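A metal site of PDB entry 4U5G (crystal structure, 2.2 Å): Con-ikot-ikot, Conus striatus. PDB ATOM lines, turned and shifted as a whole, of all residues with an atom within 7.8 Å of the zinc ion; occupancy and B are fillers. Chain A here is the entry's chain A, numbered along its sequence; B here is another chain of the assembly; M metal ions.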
ATOM      1  N   GLU A  15     -19.313  19.806  12.840  1.00  0.00           N
ATOM      2  CA  GLU A  15     -19.056  18.378  12.648  1.00  0.00           C
ATOM      3  C   GLU A  15     -20.342  17.524  12.716  1.00  0.00           C
ATOM      4  O   GLU A  15     -20.574  16.630  11.871  1.00  0.00           O
ATOM      5  CB  GLU A  15     -18.063  17.891  13.692  1.00  0.00           C
ATOM      6  CG  GLU A  15     -16.711  18.605  13.579  1.00  0.00           C
ATOM      7  CD  GLU A  15     -15.786  18.240  14.724  1.00  0.00           C
ATOM      8  OE1 GLU A  15     -16.242  17.574  15.683  1.00  0.00           O
ATOM      9  OE2 GLU A  15     -14.607  18.662  14.685  1.00  0.00           O
ATOM     10  N   CYS A  16     -21.166  17.840  13.708  1.00  0.00           N
ATOM     11  CA  CYS A  16     -22.426  17.144  13.884  1.00  0.00           C
ATOM     12  C   CYS A  16     -23.311  17.366  12.649  1.00  0.00           C
ATOM     13  O   CYS A  16     -23.912  16.435  12.131  1.00  0.00           O
ATOM     14  CB  CYS A  16     -23.123  17.638  15.160  1.00  0.00           C
ATOM     15  SG  CYS A  16     -24.855  17.158  15.452  1.00  0.00           S
ATOM     16  N   THR A  18     -22.517  18.265   9.353  1.00  0.00           N
ATOM     17  CA  THR A  18     -22.156  17.598   8.114  1.00  0.00           C
ATOM     18  C   THR A  18     -22.361  16.098   8.242  1.00  0.00           C
ATOM     19  O   THR A  18     -22.818  15.445   7.280  1.00  0.00           O
ATOM     20  CB  THR A  18     -20.712  17.908   7.706  1.00  0.00           C
ATOM     21  OG1 THR A  18     -19.822  17.390   8.703  1.00  0.00           O
ATOM     22  CG2 THR A  18     -20.495  19.406   7.585  1.00  0.00           C
ATOM     23  N   ASP A  19     -22.103  15.532   9.431  1.00  0.00           N
ATOM     24  CA  ASP A  19     -22.259  14.101   9.556  1.00  0.00           C
ATOM     25  C   ASP A  19     -23.743  13.712   9.446  1.00  0.00           C
ATOM     26  O   ASP A  19     -24.122  12.850   8.624  1.00  0.00           O
ATOM     27  CB  ASP A  19     -21.656  13.614  10.876  1.00  0.00           C
ATOM     28  CG  ASP A  19     -21.825  12.130  11.074  1.00  0.00           C
ATOM     29  OD1 ASP A  19     -21.622  11.353  10.104  1.00  0.00           O
ATOM     30  OD2 ASP A  19     -22.157  11.736  12.211  1.00  0.00           O
ATOM     31  N   ARG A  20     -24.581  14.392  10.224  1.00  0.00           N
ATOM     32  CA  ARG A  20     -26.014  14.141  10.218  1.00  0.00           C
ATOM     33  C   ARG A  20     -26.671  14.394   8.841  1.00  0.00           C
ATOM     34  O   ARG A  20     -27.538  13.618   8.422  1.00  0.00           O
ATOM     35  CB  ARG A  20     -26.683  15.003  11.309  1.00  0.00           C
ATOM     36  CG  ARG A  20     -27.240  14.223  12.507  1.00  0.00           C
ATOM     37  CD  ARG A  20     -26.386  13.006  12.888  1.00  0.00           C
ATOM     38  NE  ARG A  20     -25.218  13.352  13.689  1.00  0.00           N
ATOM     39  CZ  ARG A  20     -25.063  13.025  14.965  1.00  0.00           C
ATOM     40  NH1 ARG A  20     -25.995  12.317  15.587  1.00  0.00           N
ATOM     41  NH2 ARG A  20     -23.962  13.391  15.617  1.00  0.00           N
ATOM     42  N   ASN A  22     -25.206  14.011   6.036  1.00  0.00           N
ATOM     43  CA  ASN A  22     -24.755  12.888   5.220  1.00  0.00           C
ATOM     44  C   ASN A  22     -25.542  11.629   5.507  1.00  0.00           C
ATOM     45  O   ASN A  22     -25.966  10.928   4.572  1.00  0.00           O
ATOM     46  CB  ASN A  22     -23.250  12.629   5.451  1.00  0.00           C
ATOM     47  CG  ASN A  22     -22.685  11.553   4.539  1.00  0.00           C
ATOM     48  OD1 ASN A  22     -22.835  11.608   3.308  1.00  0.00           O
ATOM     49  ND2 ASN A  22     -21.994  10.583   5.141  1.00  0.00           N
ATOM     50  N   GLU A  23     -25.818  11.391   6.785  1.00  0.00           N
ATOM     51  CA  GLU A  23     -26.550  10.202   7.214  1.00  0.00           C
ATOM     52  C   GLU A  23     -28.033  10.263   6.822  1.00  0.00           C
ATOM     53  O   GLU A  23     -28.639   9.248   6.487  1.00  0.00           O
ATOM     54  CB  GLU A  23     -26.369  10.007   8.719  1.00  0.00           C
ATOM     55  CG  GLU A  23     -24.884   9.737   9.096  1.00  0.00           C
ATOM     56  CD  GLU A  23     -24.645   9.671  10.585  1.00  0.00           C
ATOM     57  OE1 GLU A  23     -25.283  10.476  11.303  1.00  0.00           O
ATOM     58  OE2 GLU A  23     -23.770   8.883  11.029  1.00  0.00           O
ATOM     59  N   ASN B  22     -18.430   3.848   7.550  1.00  0.00           N
ATOM     60  CA  ASN B  22     -19.819   4.267   7.832  1.00  0.00           C
ATOM     61  C   ASN B  22     -20.689   4.387   6.553  1.00  0.00           C
ATOM     62  O   ASN B  22     -21.812   3.822   6.476  1.00  0.00           O
ATOM     63  CB  ASN B  22     -19.768   5.585   8.617  1.00  0.00           C
ATOM     64  CG  ASN B  22     -21.140   6.054   9.131  1.00  0.00           C
ATOM     65  OD1 ASN B  22     -21.849   5.300   9.782  1.00  0.00           O
ATOM     66  ND2 ASN B  22     -21.449   7.334   8.904  1.00  0.00           N
ATOM     67  N   GLN B  26     -23.976   1.977   5.266  1.00  0.00           N
ATOM     68  CA  GLN B  26     -25.341   2.457   4.981  1.00  0.00           C
ATOM     69  C   GLN B  26     -25.951   1.833   3.705  1.00  0.00           C
ATOM     70  O   GLN B  26     -27.103   2.084   3.392  1.00  0.00           O
ATOM     71  CB  GLN B  26     -25.428   3.993   4.912  1.00  0.00           C
ATOM     72  CG  GLN B  26     -25.387   4.624   6.290  1.00  0.00           C
ATOM     73  CD  GLN B  26     -24.417   5.718   6.421  1.00  0.00           C
ATOM     74  OE1 GLN B  26     -23.436   5.774   5.668  1.00  0.00           O
ATOM     75  NE2 GLN B  26     -24.603   6.586   7.438  1.00  0.00           N
ATOM     76  N   TYR B  60     -10.940   0.850  15.209  1.00  0.00           N
ATOM     77  CA  TYR B  60     -12.271   1.255  14.753  1.00  0.00           C
ATOM     78  C   TYR B  60     -13.057   0.019  14.326  1.00  0.00           C
ATOM     79  O   TYR B  60     -14.237  -0.090  14.632  1.00  0.00           O
ATOM     80  CB  TYR B  60     -12.181   2.277  13.602  1.00  0.00           C
ATOM     81  CG  TYR B  60     -13.544   2.762  13.114  1.00  0.00           C
ATOM     82  CD1 TYR B  60     -14.326   3.600  13.906  1.00  0.00           C
ATOM     83  CD2 TYR B  60     -14.041   2.408  11.860  1.00  0.00           C
ATOM     84  CE1 TYR B  60     -15.563   4.057  13.477  1.00  0.00           C
ATOM     85  CE2 TYR B  60     -15.283   2.862  11.412  1.00  0.00           C
ATOM     86  CZ  TYR B  60     -16.041   3.688  12.229  1.00  0.00           C
ATOM     87  OH  TYR B  60     -17.265   4.142  11.806  1.00  0.00           O
ATOM     88  N   LEU B  73     -26.902   1.970  12.971  1.00  0.00           N
ATOM     89  CA  LEU B  73     -25.579   2.420  12.531  1.00  0.00           C
ATOM     90  C   LEU B  73     -25.098   3.762  13.108  1.00  0.00           C
ATOM     91  O   LEU B  73     -23.985   3.839  13.613  1.00  0.00           O
ATOM     92  CB  LEU B  73     -25.526   2.466  11.001  1.00  0.00           C
ATOM     93  CG  LEU B  73     -24.176   2.901  10.396  1.00  0.00           C
ATOM     94  CD1 LEU B  73     -23.032   2.064  10.917  1.00  0.00           C
ATOM     95  CD2 LEU B  73     -24.269   2.785   8.893  1.00  0.00           C
ATOM     96  N   SER B  74     -25.921   4.801  13.017  1.00  0.00           N
ATOM     97  CA  SER B  74     -25.550   6.141  13.481  1.00  0.00           C
ATOM     98  C   SER B  74     -24.971   6.148  14.892  1.00  0.00           C
ATOM     99  O   SER B  74     -23.904   6.739  15.132  1.00  0.00           O
ATOM    100  CB  SER B  74     -26.778   7.046  13.445  1.00  0.00           C
ATOM    101  OG  SER B  74     -26.524   8.289  14.067  1.00  0.00           O
ATOM    102  N   GLY B  75     -25.629   5.444  15.816  1.00  0.00           N
ATOM    103  CA  GLY B  75     -25.159   5.316  17.185  1.00  0.00           C
ATOM    104  C   GLY B  75     -23.754   4.741  17.268  1.00  0.00           C
ATOM    105  O   GLY B  75     -22.935   5.159  18.111  1.00  0.00           O
ATOM    106  N   ALA B  76     -23.477   3.787  16.381  1.00  0.00           N
ATOM    107  CA  ALA B  76     -22.164   3.157  16.331  1.00  0.00           C
ATOM    108  C   ALA B  76     -21.139   4.157  15.789  1.00  0.00           C
ATOM    109  O   ALA B  76     -20.023   4.213  16.296  1.00  0.00           O
ATOM    110  CB  ALA B  76     -22.175   1.905  15.514  1.00  0.00           C
ATOM    111  N   HIS B  77     -21.518   4.906  14.742  1.00  0.00           N
ATOM    112  CA  HIS B  77     -20.617   5.941  14.225  1.00  0.00           C
ATOM    113  C   HIS B  77     -20.214   6.854  15.382  1.00  0.00           C
ATOM    114  O   HIS B  77     -19.029   7.032  15.639  1.00  0.00           O
ATOM    115  CB  HIS B  77     -21.276   6.779  13.121  1.00  0.00           C
ATOM    116  CG  HIS B  77     -20.308   7.648  12.360  1.00  0.00           C
ATOM    117  ND1 HIS B  77     -20.508   8.993  12.151  1.00  0.00           N
ATOM    118  CD2 HIS B  77     -19.108   7.350  11.783  1.00  0.00           C
ATOM    119  CE1 HIS B  77     -19.496   9.490  11.478  1.00  0.00           C
ATOM    120  NE2 HIS B  77     -18.627   8.518  11.238  1.00  0.00           N
ATOM    121  N   GLU B  78     -21.194   7.415  16.096  1.00  0.00           N
ATOM    122  CA  GLU B  78     -20.903   8.356  17.170  1.00  0.00           C
ATOM    123  C   GLU B  78     -20.109   7.719  18.309  1.00  0.00           C
ATOM    124  O   GLU B  78     -19.301   8.385  18.953  1.00  0.00           O
ATOM    125  CB  GLU B  78     -22.195   9.002  17.677  1.00  0.00           C
ATOM    126  CG  GLU B  78     -22.480  10.340  17.010  1.00  0.00           C
ATOM    127  CD  GLU B  78     -22.331  10.291  15.483  1.00  0.00           C
ATOM    128  OE1 GLU B  78     -21.330  10.827  14.956  1.00  0.00           O
ATOM    129  OE2 GLU B  78     -23.223   9.711  14.812  1.00  0.00           O
ATOM    130  N   ALA B  79     -20.294   6.429  18.530  1.00  0.00           N
ATOM    131  CA  ALA B  79     -19.588   5.784  19.604  1.00  0.00           C
ATOM    132  C   ALA B  79     -18.131   5.437  19.268  1.00  0.00           C
ATOM    133  O   ALA B  79     -17.259   5.521  20.138  1.00  0.00           O
ATOM    134  CB  ALA B  79     -20.321   4.518  19.980  1.00  0.00           C
ATOM    135  N   LYS B  81     -16.129   6.553  16.375  1.00  0.00           N
ATOM    136  CA  LYS B  81     -15.304   7.358  15.468  1.00  0.00           C
ATOM    137  C   LYS B  81     -14.044   7.960  16.110  1.00  0.00           C
ATOM    138  O   LYS B  81     -13.056   8.167  15.409  1.00  0.00           O
ATOM    139  CB  LYS B  81     -16.146   8.446  14.793  1.00  0.00           C
ATOM    140  CG  LYS B  81     -16.787   9.552  15.589  1.00  0.00           C
ATOM    141  CD  LYS B  81     -17.627  10.375  14.577  1.00  0.00           C
ATOM    142  CE  LYS B  81     -18.390  11.569  15.167  1.00  0.00           C
ATOM    143  NZ  LYS B  81     -19.125  12.340  14.086  1.00  0.00           N
HETATM  144 ZN    ZN M   1     -22.418   9.895  12.467  1.00  0.00          ZN
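NH2 of Arg 20 is in salt-bridge range of OE1 of Glu 78 of chain B (3.7 Å).
NZ of Lys 81 of chain B lies within salt-bridge range of OE1 of Glu 78 of chain B (2.8 Å).
The side-chain carboxylate (OD2) of Asp 19 lies close to the side-chain amino group (NZ) of Lys 81 of chain B, at 3.6 Å.
OD2 of Asp 19 lies close to NE of Arg 20 (3.8 Å).
The side-chain carboxylate (OE1) of Glu 23 is in salt-bridge range of the guanidinium group (NE) of Arg 20, at 3.7 Å.
Four residues have an atom within 4 Å of the zinc ion: Asp 19, Glu 23, His 77 of chain B and Glu 78 of chain B.
The zinc ion is bound by the side-chain carboxylate (OD2) of Asp 19 (1.9 Å), a ring nitrogen (ND1) of His 77 of chain B (2.1 Å), the side-chain carboxylate (OE2) of Glu 23 (2.2 Å) and the side-chain carboxylate (OE2) of Glu 78 of chain B (2.5 Å).
The zinc ion has four donor atoms within binding distance.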
